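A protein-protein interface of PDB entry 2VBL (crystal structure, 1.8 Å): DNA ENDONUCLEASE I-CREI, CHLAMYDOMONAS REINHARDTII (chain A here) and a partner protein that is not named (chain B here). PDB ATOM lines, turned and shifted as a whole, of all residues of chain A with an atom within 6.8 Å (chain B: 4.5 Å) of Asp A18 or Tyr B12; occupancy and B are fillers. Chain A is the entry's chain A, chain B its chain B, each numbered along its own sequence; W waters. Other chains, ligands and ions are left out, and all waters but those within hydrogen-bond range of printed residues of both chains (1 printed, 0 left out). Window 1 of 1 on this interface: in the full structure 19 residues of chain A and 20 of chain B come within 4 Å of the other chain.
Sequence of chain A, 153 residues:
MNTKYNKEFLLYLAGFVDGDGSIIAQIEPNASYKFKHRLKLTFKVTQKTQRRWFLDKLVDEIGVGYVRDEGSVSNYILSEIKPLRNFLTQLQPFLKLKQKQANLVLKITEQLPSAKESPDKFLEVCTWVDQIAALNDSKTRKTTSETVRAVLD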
ATOM      1  N   GLU A   8       5.474   8.531  17.443  1.00  0.00           N
ATOM      2  CA  GLU A   8       4.536   9.633  17.675  1.00  0.00           C
ATOM      3  C   GLU A   8       3.945  10.149  16.368  1.00  0.00           C
ATOM      4  O   GLU A   8       2.810  10.611  16.343  1.00  0.00           O
ATOM      5  CB  GLU A   8       5.181  10.800  18.436  1.00  0.00           C
ATOM      6  CG  GLU A   8       5.706  10.427  19.829  1.00  0.00           C
ATOM      7  CD  GLU A   8       5.966  11.652  20.704  1.00  0.00           C
ATOM      8  OE1 GLU A   8       5.647  12.791  20.277  1.00  0.00           O
ATOM      9  OE2 GLU A   8       6.488  11.487  21.832  1.00  0.00           O
ATOM     10  N   LEU A  10       3.459   8.183  13.651  1.00  0.00           N
ATOM     11  CA  LEU A  10       2.520   7.165  13.179  1.00  0.00           C
ATOM     12  C   LEU A  10       1.188   7.248  13.934  1.00  0.00           C
ATOM     13  O   LEU A  10       0.112   7.082  13.340  1.00  0.00           O
ATOM     14  CB  LEU A  10       3.113   5.751  13.276  1.00  0.00           C
ATOM     15  CG  LEU A  10       4.332   5.544  12.387  1.00  0.00           C
ATOM     16  CD1 LEU A  10       5.066   4.257  12.868  1.00  0.00           C
ATOM     17  CD2 LEU A  10       3.893   5.424  10.916  1.00  0.00           C
ATOM     18  N   LEU A  11       1.265   7.482  15.245  1.00  0.00           N
ATOM     19  CA  LEU A  11       0.042   7.604  16.043  1.00  0.00           C
ATOM     20  C   LEU A  11      -0.850   8.780  15.579  1.00  0.00           C
ATOM     21  O   LEU A  11      -2.071   8.614  15.384  1.00  0.00           O
ATOM     22  CB  LEU A  11       0.433   7.812  17.502  1.00  0.00           C
ATOM     23  CG  LEU A  11       0.767   6.513  18.245  1.00  0.00           C
ATOM     24  CD1 LEU A  11       1.550   6.834  19.553  1.00  0.00           C
ATOM     25  CD2 LEU A  11      -0.556   5.791  18.566  1.00  0.00           C
ATOM     26  N   TYR A  12      -0.248   9.962  15.509  1.00  0.00           N
ATOM     27  CA  TYR A  12      -0.949  11.136  14.967  1.00  0.00           C
ATOM     28  C   TYR A  12      -1.475  10.897  13.551  1.00  0.00           C
ATOM     29  O   TYR A  12      -2.647  11.150  13.241  1.00  0.00           O
ATOM     30  CB  TYR A  12      -0.039  12.383  15.025  1.00  0.00           C
ATOM     31  CG  TYR A  12      -0.707  13.573  14.339  1.00  0.00           C
ATOM     32  CD1 TYR A  12      -1.390  14.534  15.085  1.00  0.00           C
ATOM     33  CD2 TYR A  12      -0.671  13.679  12.955  1.00  0.00           C
ATOM     34  CE1 TYR A  12      -2.070  15.603  14.446  1.00  0.00           C
ATOM     35  CE2 TYR A  12      -1.315  14.765  12.291  1.00  0.00           C
ATOM     36  CZ  TYR A  12      -1.989  15.722  13.056  1.00  0.00           C
ATOM     37  OH  TYR A  12      -2.636  16.760  12.407  1.00  0.00           O
ATOM     38  N   LEU A  13      -0.619  10.389  12.680  1.00  0.00           N
ATOM     39  CA  LEU A  13      -1.027  10.165  11.289  1.00  0.00           C
ATOM     40  C   LEU A  13      -2.112   9.098  11.189  1.00  0.00           C
ATOM     41  O   LEU A  13      -2.954   9.183  10.311  1.00  0.00           O
ATOM     42  CB  LEU A  13       0.171   9.730  10.440  1.00  0.00           C
ATOM     43  CG  LEU A  13      -0.109   9.579   8.935  1.00  0.00           C
ATOM     44  CD1 LEU A  13      -0.711  10.884   8.332  1.00  0.00           C
ATOM     45  CD2 LEU A  13       1.189   9.219   8.194  1.00  0.00           C
ATOM     46  N   ALA A  14      -2.072   8.072  12.045  1.00  0.00           N
ATOM     47  CA  ALA A  14      -3.118   7.053  11.992  1.00  0.00           C
ATOM     48  C   ALA A  14      -4.463   7.720  12.288  1.00  0.00           C
ATOM     49  O   ALA A  14      -5.465   7.423  11.627  1.00  0.00           O
ATOM     50  CB  ALA A  14      -2.864   5.976  13.000  1.00  0.00           C
ATOM     51  N   GLY A  15      -4.490   8.600  13.289  1.00  0.00           N
ATOM     52  CA  GLY A  15      -5.718   9.355  13.607  1.00  0.00           C
ATOM     53  C   GLY A  15      -6.134  10.215  12.423  1.00  0.00           C
ATOM     54  O   GLY A  15      -7.340  10.246  12.030  1.00  0.00           O
ATOM     55  N   PHE A  16      -5.163  10.923  11.826  1.00  0.00           N
ATOM     56  CA  PHE A  16      -5.530  11.866  10.745  1.00  0.00           C
ATOM     57  C   PHE A  16      -6.054  11.078   9.532  1.00  0.00           C
ATOM     58  O   PHE A  16      -7.007  11.502   8.821  1.00  0.00           O
ATOM     59  CB  PHE A  16      -4.346  12.747  10.305  1.00  0.00           C
ATOM     60  CG  PHE A  16      -4.771  13.945   9.514  1.00  0.00           C
ATOM     61  CD1 PHE A  16      -5.153  15.110  10.173  1.00  0.00           C
ATOM     62  CD2 PHE A  16      -4.875  13.885   8.100  1.00  0.00           C
ATOM     63  CE1 PHE A  16      -5.614  16.237   9.428  1.00  0.00           C
ATOM     64  CE2 PHE A  16      -5.310  15.033   7.374  1.00  0.00           C
ATOM     65  CZ  PHE A  16      -5.658  16.179   8.068  1.00  0.00           C
ATOM     66  N   VAL A  17      -5.473   9.904   9.307  1.00  0.00           N
ATOM     67  CA  VAL A  17      -5.891   9.022   8.212  1.00  0.00           C
ATOM     68  C   VAL A  17      -7.272   8.436   8.401  1.00  0.00           C
ATOM     69  O   VAL A  17      -8.090   8.399   7.467  1.00  0.00           O
ATOM     70  CB  VAL A  17      -4.839   7.903   7.983  1.00  0.00           C
ATOM     71  CG1 VAL A  17      -5.396   6.785   7.063  1.00  0.00           C
ATOM     72  CG2 VAL A  17      -3.593   8.554   7.357  1.00  0.00           C
ATOM     73  N   ASP A  18      -7.558   7.979   9.601  1.00  0.00           N
ATOM     74  CA  ASP A  18      -8.866   7.407   9.902  1.00  0.00           C
ATOM     75  C   ASP A  18      -9.905   8.497   9.672  1.00  0.00           C
ATOM     76  O   ASP A  18     -11.043   8.218   9.258  1.00  0.00           O
ATOM     77  CB  ASP A  18      -8.911   6.957  11.371  1.00  0.00           C
ATOM     78  CG  ASP A  18      -8.423   5.526  11.575  1.00  0.00           C
ATOM     79  OD1 ASP A  18      -8.359   4.749  10.592  1.00  0.00           O
ATOM     80  OD2 ASP A  18      -8.126   5.174  12.738  1.00  0.00           O
ATOM     81  N   GLY A  19      -9.521   9.753   9.873  1.00  0.00           N
ATOM     82  CA  GLY A  19     -10.465  10.871   9.593  1.00  0.00           C
ATOM     83  C   GLY A  19     -10.556  11.300   8.138  1.00  0.00           C
ATOM     84  O   GLY A  19     -11.640  11.173   7.544  1.00  0.00           O
ATOM     85  N   ASP A  20      -9.456  11.802   7.554  1.00  0.00           N
ATOM     86  CA  ASP A  20      -9.504  12.440   6.204  1.00  0.00           C
ATOM     87  C   ASP A  20      -8.813  11.636   5.090  1.00  0.00           C
ATOM     88  O   ASP A  20      -8.675  12.120   3.950  1.00  0.00           O
ATOM     89  CB  ASP A  20      -8.831  13.818   6.226  1.00  0.00           C
ATOM     90  CG  ASP A  20      -9.689  14.913   6.837  1.00  0.00           C
ATOM     91  OD1 ASP A  20     -10.913  14.766   6.914  1.00  0.00           O
ATOM     92  OD2 ASP A  20      -9.134  15.985   7.190  1.00  0.00           O
ATOM     93  N   GLY A  21      -8.316  10.443   5.436  1.00  0.00           N
ATOM     94  CA  GLY A  21      -7.590   9.604   4.512  1.00  0.00           C
ATOM     95  C   GLY A  21      -8.484   8.581   3.829  1.00  0.00           C
ATOM     96  O   GLY A  21      -9.673   8.416   4.156  1.00  0.00           O
ATOM     97  N   SER A  22      -7.899   7.857   2.890  1.00  0.00           N
ATOM     98  CA  SER A  22      -8.651   6.872   2.132  1.00  0.00           C
ATOM     99  C   SER A  22      -7.653   5.772   1.714  1.00  0.00           C
ATOM    100  O   SER A  22      -6.558   6.081   1.234  1.00  0.00           O
ATOM    101  CB  SER A  22      -9.278   7.557   0.911  1.00  0.00           C
ATOM    102  OG  SER A  22     -10.203   6.661   0.298  1.00  0.00           O
ATOM    103  N   PHE A  94      -1.821   1.140  14.331  1.00  0.00           N
ATOM    104  CA  PHE A  94      -2.337   2.324  15.037  1.00  0.00           C
ATOM    105  C   PHE A  94      -3.673   2.776  14.469  1.00  0.00           C
ATOM    106  O   PHE A  94      -4.342   3.652  15.037  1.00  0.00           O
ATOM    107  CB  PHE A  94      -1.315   3.472  14.999  1.00  0.00           C
ATOM    108  CG  PHE A  94       0.007   3.098  15.604  1.00  0.00           C
ATOM    109  CD1 PHE A  94       0.113   2.935  16.976  1.00  0.00           C
ATOM    110  CD2 PHE A  94       1.103   2.859  14.798  1.00  0.00           C
ATOM    111  CE1 PHE A  94       1.337   2.536  17.560  1.00  0.00           C
ATOM    112  CE2 PHE A  94       2.338   2.477  15.374  1.00  0.00           C
ATOM    113  CZ  PHE A  94       2.432   2.325  16.748  1.00  0.00           C
ATOM    114  N   LEU A  95      -4.044   2.220  13.323  1.00  0.00           N
ATOM    115  CA  LEU A  95      -5.358   2.499  12.733  1.00  0.00           C
ATOM    116  C   LEU A  95      -6.491   1.900  13.569  1.00  0.00           C
ATOM    117  O   LEU A  95      -6.388   0.758  14.060  1.00  0.00           O
ATOM    118  CB  LEU A  95      -5.454   1.969  11.290  1.00  0.00           C
ATOM    119  CG  LEU A  95      -4.532   2.674  10.285  1.00  0.00           C
ATOM    120  CD1 LEU A  95      -4.529   1.943   8.939  1.00  0.00           C
ATOM    121  CD2 LEU A  95      -4.961   4.169  10.106  1.00  0.00           C
ATOM    122  N   LYS A  96      -7.594   2.648  13.669  1.00  0.00           N
ATOM    123  CA  LYS A  96      -8.788   2.195  14.373  1.00  0.00           C
ATOM    124  C   LYS A  96     -10.004   2.001  13.473  1.00  0.00           C
ATOM    125  O   LYS A  96     -10.827   1.103  13.731  1.00  0.00           O
ATOM    126  CB  LYS A  96      -9.134   3.161  15.519  1.00  0.00           C
ATOM    127  CG  LYS A  96      -8.056   3.172  16.604  1.00  0.00           C
ATOM    128  CD  LYS A  96      -8.484   4.090  17.752  1.00  0.00           C
ATOM    129  CE  LYS A  96      -7.366   4.316  18.747  1.00  0.00           C
ATOM    130  NZ  LYS A  96      -7.885   4.944  20.010  1.00  0.00           N
ATOM    131  N   LEU A  97     -10.147   2.845  12.450  1.00  0.00           N
ATOM    132  CA  LEU A  97     -11.263   2.695  11.497  1.00  0.00           C
ATOM    133  C   LEU A  97     -10.843   1.956  10.243  1.00  0.00           C
ATOM    134  O   LEU A  97     -11.678   1.258   9.656  1.00  0.00           O
ATOM    135  CB  LEU A  97     -11.849   4.050  11.070  1.00  0.00           C
ATOM    136  CG  LEU A  97     -12.460   4.838  12.226  1.00  0.00           C
ATOM    137  CD1 LEU A  97     -12.994   6.227  11.803  1.00  0.00           C
ATOM    138  CD2 LEU A  97     -13.522   3.982  12.947  1.00  0.00           C
ATOM    139  N   LYS A  98      -9.584   2.142   9.823  1.00  0.00           N
ATOM    140  CA  LYS A  98      -9.105   1.666   8.517  1.00  0.00           C
ATOM    141  C   LYS A  98      -8.107   0.508   8.625  1.00  0.00           C
ATOM    142  O   LYS A  98      -7.388   0.177   7.683  1.00  0.00           O
ATOM    143  CB  LYS A  98      -8.571   2.837   7.683  1.00  0.00           C
ATOM    144  CG  LYS A  98      -9.684   3.850   7.390  1.00  0.00           C
ATOM    145  CD  LYS A  98      -9.210   4.928   6.430  1.00  0.00           C
ATOM    146  CE  LYS A  98     -10.167   6.103   6.476  1.00  0.00           C
ATOM    147  NZ  LYS A  98     -11.236   5.927   5.480  1.00  0.00           N
ATOM    148  N   GLN A  99      -8.076  -0.133   9.783  1.00  0.00           N
ATOM    149  CA  GLN A  99      -7.086  -1.200   9.974  1.00  0.00           C
ATOM    150  C   GLN A  99      -7.342  -2.382   9.024  1.00  0.00           C
ATOM    151  O   GLN A  99      -6.419  -2.916   8.403  1.00  0.00           O
ATOM    152  CB  GLN A  99      -7.050  -1.634  11.426  1.00  0.00           C
ATOM    153  CG  GLN A  99      -5.748  -2.323  11.812  1.00  0.00           C
ATOM    154  CD  GLN A  99      -5.715  -2.691  13.274  1.00  0.00           C
ATOM    155  OE1 GLN A  99      -6.588  -3.421  13.744  1.00  0.00           O
ATOM    156  NE2 GLN A  99      -4.733  -2.174  14.008  1.00  0.00           N
ATOM    157  N   GLU B   8      -0.461   8.257  24.270  1.00  0.00           N
ATOM    158  CA  GLU B   8      -0.769   7.646  22.959  1.00  0.00           C
ATOM    159  C   GLU B   8      -2.204   7.875  22.525  1.00  0.00           C
ATOM    160  O   GLU B   8      -2.466   8.073  21.330  1.00  0.00           O
ATOM    161  CB  GLU B   8      -0.469   6.156  22.961  1.00  0.00           C
ATOM    162  CG  GLU B   8       1.004   5.915  23.229  1.00  0.00           C
ATOM    163  CD  GLU B   8       1.440   4.496  22.903  1.00  0.00           C
ATOM    164  OE1 GLU B   8       0.688   3.746  22.251  1.00  0.00           O
ATOM    165  OE2 GLU B   8       2.557   4.130  23.310  1.00  0.00           O
ATOM    166  N   PHE B   9      -3.110   7.867  23.496  1.00  0.00           N
ATOM    167  CA  PHE B   9      -4.486   8.262  23.234  1.00  0.00           C
ATOM    168  C   PHE B   9      -4.569   9.696  22.696  1.00  0.00           C
ATOM    169  O   PHE B   9      -5.288   9.974  21.709  1.00  0.00           O
ATOM    170  CB  PHE B   9      -5.308   8.095  24.505  1.00  0.00           C
ATOM    171  CG  PHE B   9      -6.617   8.859  24.503  1.00  0.00           C
ATOM    172  CD1 PHE B   9      -7.723   8.357  23.845  1.00  0.00           C
ATOM    173  CD2 PHE B   9      -6.739  10.081  25.176  1.00  0.00           C
ATOM    174  CE1 PHE B   9      -8.937   9.068  23.855  1.00  0.00           C
ATOM    175  CE2 PHE B   9      -7.943  10.767  25.217  1.00  0.00           C
ATOM    176  CZ  PHE B   9      -9.042  10.258  24.556  1.00  0.00           C
ATOM    177  N   LEU B  10      -3.881  10.617  23.357  1.00  0.00           N
ATOM    178  CA  LEU B  10      -3.949  12.033  22.921  1.00  0.00           C
ATOM    179  C   LEU B  10      -3.330  12.235  21.540  1.00  0.00           C
ATOM    180  O   LEU B  10      -3.811  13.041  20.739  1.00  0.00           O
ATOM    181  CB  LEU B  10      -3.221  12.936  23.931  1.00  0.00           C
ATOM    182  CG  LEU B  10      -3.896  13.046  25.293  1.00  0.00           C
ATOM    183  CD1 LEU B  10      -2.992  13.729  26.314  1.00  0.00           C
ATOM    184  CD2 LEU B  10      -5.221  13.843  25.181  1.00  0.00           C
ATOM    185  N   LEU B  11      -2.244  11.518  21.253  1.00  0.00           N
ATOM    186  CA  LEU B  11      -1.588  11.613  19.942  1.00  0.00           C
ATOM    187  C   LEU B  11      -2.524  11.185  18.833  1.00  0.00           C
ATOM    188  O   LEU B  11      -2.681  11.922  17.856  1.00  0.00           O
ATOM    189  CB  LEU B  11      -0.315  10.740  19.876  1.00  0.00           C
ATOM    190  CG  LEU B  11       0.876  11.514  20.436  1.00  0.00           C
ATOM    191  CD1 LEU B  11       1.986  10.473  20.860  1.00  0.00           C
ATOM    192  CD2 LEU B  11       1.429  12.491  19.380  1.00  0.00           C
ATOM    193  N   TYR B  12      -3.089   9.978  18.955  1.00  0.00           N
ATOM    194  CA  TYR B  12      -4.043   9.515  17.958  1.00  0.00           C
ATOM    195  C   TYR B  12      -5.230  10.481  17.856  1.00  0.00           C
ATOM    196  O   TYR B  12      -5.687  10.818  16.745  1.00  0.00           O
ATOM    197  CB  TYR B  12      -4.547   8.101  18.317  1.00  0.00           C
ATOM    198  CG  TYR B  12      -5.641   7.632  17.371  1.00  0.00           C
ATOM    199  CD1 TYR B  12      -5.345   6.899  16.218  1.00  0.00           C
ATOM    200  CD2 TYR B  12      -6.977   7.993  17.605  1.00  0.00           C
ATOM    201  CE1 TYR B  12      -6.372   6.520  15.329  1.00  0.00           C
ATOM    202  CE2 TYR B  12      -7.986   7.646  16.735  1.00  0.00           C
ATOM    203  CZ  TYR B  12      -7.702   6.909  15.617  1.00  0.00           C
ATOM    204  OH  TYR B  12      -8.757   6.603  14.783  1.00  0.00           O
ATOM    205  N   LEU B  13      -5.776  10.896  19.001  1.00  0.00           N
ATOM    206  CA  LEU B  13      -6.997  11.699  18.977  1.00  0.00           C
ATOM    207  C   LEU B  13      -6.680  13.054  18.358  1.00  0.00           C
ATOM    208  O   LEU B  13      -7.504  13.642  17.644  1.00  0.00           O
ATOM    209  CB  LEU B  13      -7.574  11.856  20.384  1.00  0.00           C
ATOM    210  CG  LEU B  13      -8.880  12.660  20.480  1.00  0.00           C
ATOM    211  CD1 LEU B  13      -9.986  12.072  19.549  1.00  0.00           C
ATOM    212  CD2 LEU B  13      -9.308  12.674  21.937  1.00  0.00           C
ATOM    213  N   ALA B  14      -5.500  13.592  18.626  1.00  0.00           N
ATOM    214  CA  ALA B  14      -5.151  14.871  17.983  1.00  0.00           C
ATOM    215  C   ALA B  14      -5.193  14.779  16.435  1.00  0.00           C
ATOM    216  O   ALA B  14      -5.707  15.692  15.736  1.00  0.00           O
ATOM    217  CB  ALA B  14      -3.759  15.340  18.479  1.00  0.00           C
ATOM    218  N   GLY B  15      -4.673  13.682  15.881  1.00  0.00           N
ATOM    219  CA  GLY B  15      -4.771  13.458  14.437  1.00  0.00           C
ATOM    220  C   GLY B  15      -6.222  13.382  14.007  1.00  0.00           C
ATOM    221  O   GLY B  15      -6.634  14.010  13.011  1.00  0.00           O
ATOM    222  N   PHE B  16      -7.019  12.605  14.731  1.00  0.00           N
ATOM    223  CA  PHE B  16      -8.424  12.428  14.311  1.00  0.00           C
ATOM    224  C   PHE B  16      -9.210  13.746  14.385  1.00  0.00           C
ATOM    225  O   PHE B  16     -10.041  14.046  13.522  1.00  0.00           O
ATOM    226  CB  PHE B  16      -9.115  11.378  15.185  1.00  0.00           C
ATOM    227  CG  PHE B  16     -10.372  10.841  14.569  1.00  0.00           C
ATOM    228  CD1 PHE B  16     -10.295   9.782  13.658  1.00  0.00           C
ATOM    229  CD2 PHE B  16     -11.613  11.421  14.824  1.00  0.00           C
ATOM    230  CE1 PHE B  16     -11.440   9.293  13.035  1.00  0.00           C
ATOM    231  CE2 PHE B  16     -12.766  10.918  14.214  1.00  0.00           C
ATOM    232  CZ  PHE B  16     -12.690   9.878  13.319  1.00  0.00           C
ATOM    233  N   PHE B  54     -17.593   4.411  17.521  1.00  0.00           N
ATOM    234  CA  PHE B  54     -16.293   5.045  17.705  1.00  0.00           C
ATOM    235  C   PHE B  54     -16.470   6.296  18.575  1.00  0.00           C
ATOM    236  O   PHE B  54     -15.685   6.569  19.479  1.00  0.00           O
ATOM    237  CB  PHE B  54     -15.735   5.387  16.315  1.00  0.00           C
ATOM    238  CG  PHE B  54     -14.439   6.168  16.322  1.00  0.00           C
ATOM    239  CD1 PHE B  54     -13.233   5.519  16.169  1.00  0.00           C
ATOM    240  CD2 PHE B  54     -14.441   7.557  16.390  1.00  0.00           C
ATOM    241  CE1 PHE B  54     -12.040   6.226  16.135  1.00  0.00           C
ATOM    242  CE2 PHE B  54     -13.258   8.280  16.382  1.00  0.00           C
ATOM    243  CZ  PHE B  54     -12.048   7.604  16.257  1.00  0.00           C
HETATM  244  O   HOH W   1      -7.179   7.993  20.688  1.00  0.00           O
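OD2 of Asp A18 lies within hydrogen-bond range of N of Lys A96, at 2.7 Å. The backbone NH (N) of Leu A97 is in hydrogen-bond range of the side-chain carboxylate (OD2) of Asp A18 (3.1 Å). The backbone NH (N) of Lys A98 sits at hydrogen-bond distance from the side-chain carboxylate (OD1) of Asp A18, at 3.0 Å.
Printed residues of chain B within 4 Å of Gly A15: Tyr B12, Gly B15 and Phe B16. Asp A18 touches two residues of chain B. Of the printed residues of chain A, Tyr B12 touches Leu A11 (3.4 Å), Ala A14 (3.8 Å), Gly A15 (3.4 Å), Asp A18 (2.6 Å), Phe A94 (3.5 Å) and Lys A96 (3.5 Å). Of the printed residues of chain A, Ala B14 touches Tyr A12. The nearest printed residue of chain B that does not touch Asp A18 is Phe B54 (5.3 Å). The nearest residue of chain A that does not touch Tyr B12 is Tyr A12 (4.5 Å). The nearest printed residue of chain A that does not touch Glu B8 is Phe A94 (4.9 Å).
Among the printed residues, merely in contact across the chains: Glu A8 with Leu B11 (3.8 Å), Leu A11 with Glu B8 (3.8 Å), Leu A11 with Leu B11 (3.8 Å), Leu A11 with Tyr B12 (3.4 Å), Tyr A12 with Leu B11 (3.5 Å), Tyr A12 with Ala B14 (3.8 Å), Tyr A12 with Gly B15 (3.4 Å), Ala A14 with Tyr B12 (3.8 Å), Gly A15 with Tyr B12 (3.4 Å), Gly A15 with Gly B15 (3.5 Å), Gly A15 with Phe B16 (3.3 Å), Phe A16 with Gly B15 (3.3 Å), Phe A16 with Phe B16 (3.8 Å), Asp A18 with Phe B16 (3.8 Å), Gly A19 with Phe B16 (3.7 Å), Phe A94 with Tyr B12 (3.5 Å), Lys A96 with Tyr B12 (3.5 Å), Leu A97 with Phe B16 (3.7 Å) and Leu A97 with Phe B54 (3.6 Å).
Water W1 bridges the backbone carbonyl oxygen of Phe B9 (2.9 Å) and the side-chain amino group of Lys A96 (3.2 Å).
The side-chain carboxylate (OD2) of Asp A18 sits at hydrogen-bond distance from the side-chain hydroxyl (OH) of Tyr B12.
Printed residues of chain A that touch a printed residue of chain B: Glu A8, Leu A11, Tyr A12, Ala A14, Gly A15, Phe A16, Asp A18, Gly A19, Phe A94, Lys A96 and Leu A97. Hydrophobic or aromatic side chains of chain B within 4 Å of the printed part of chain A: Leu B11, Tyr B12, Phe B16 and Phe B54. Among the printed residues, no Asp or Glu carboxylate lies within 4 Å of a Lys or Arg side-chain nitrogen of the other chain.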
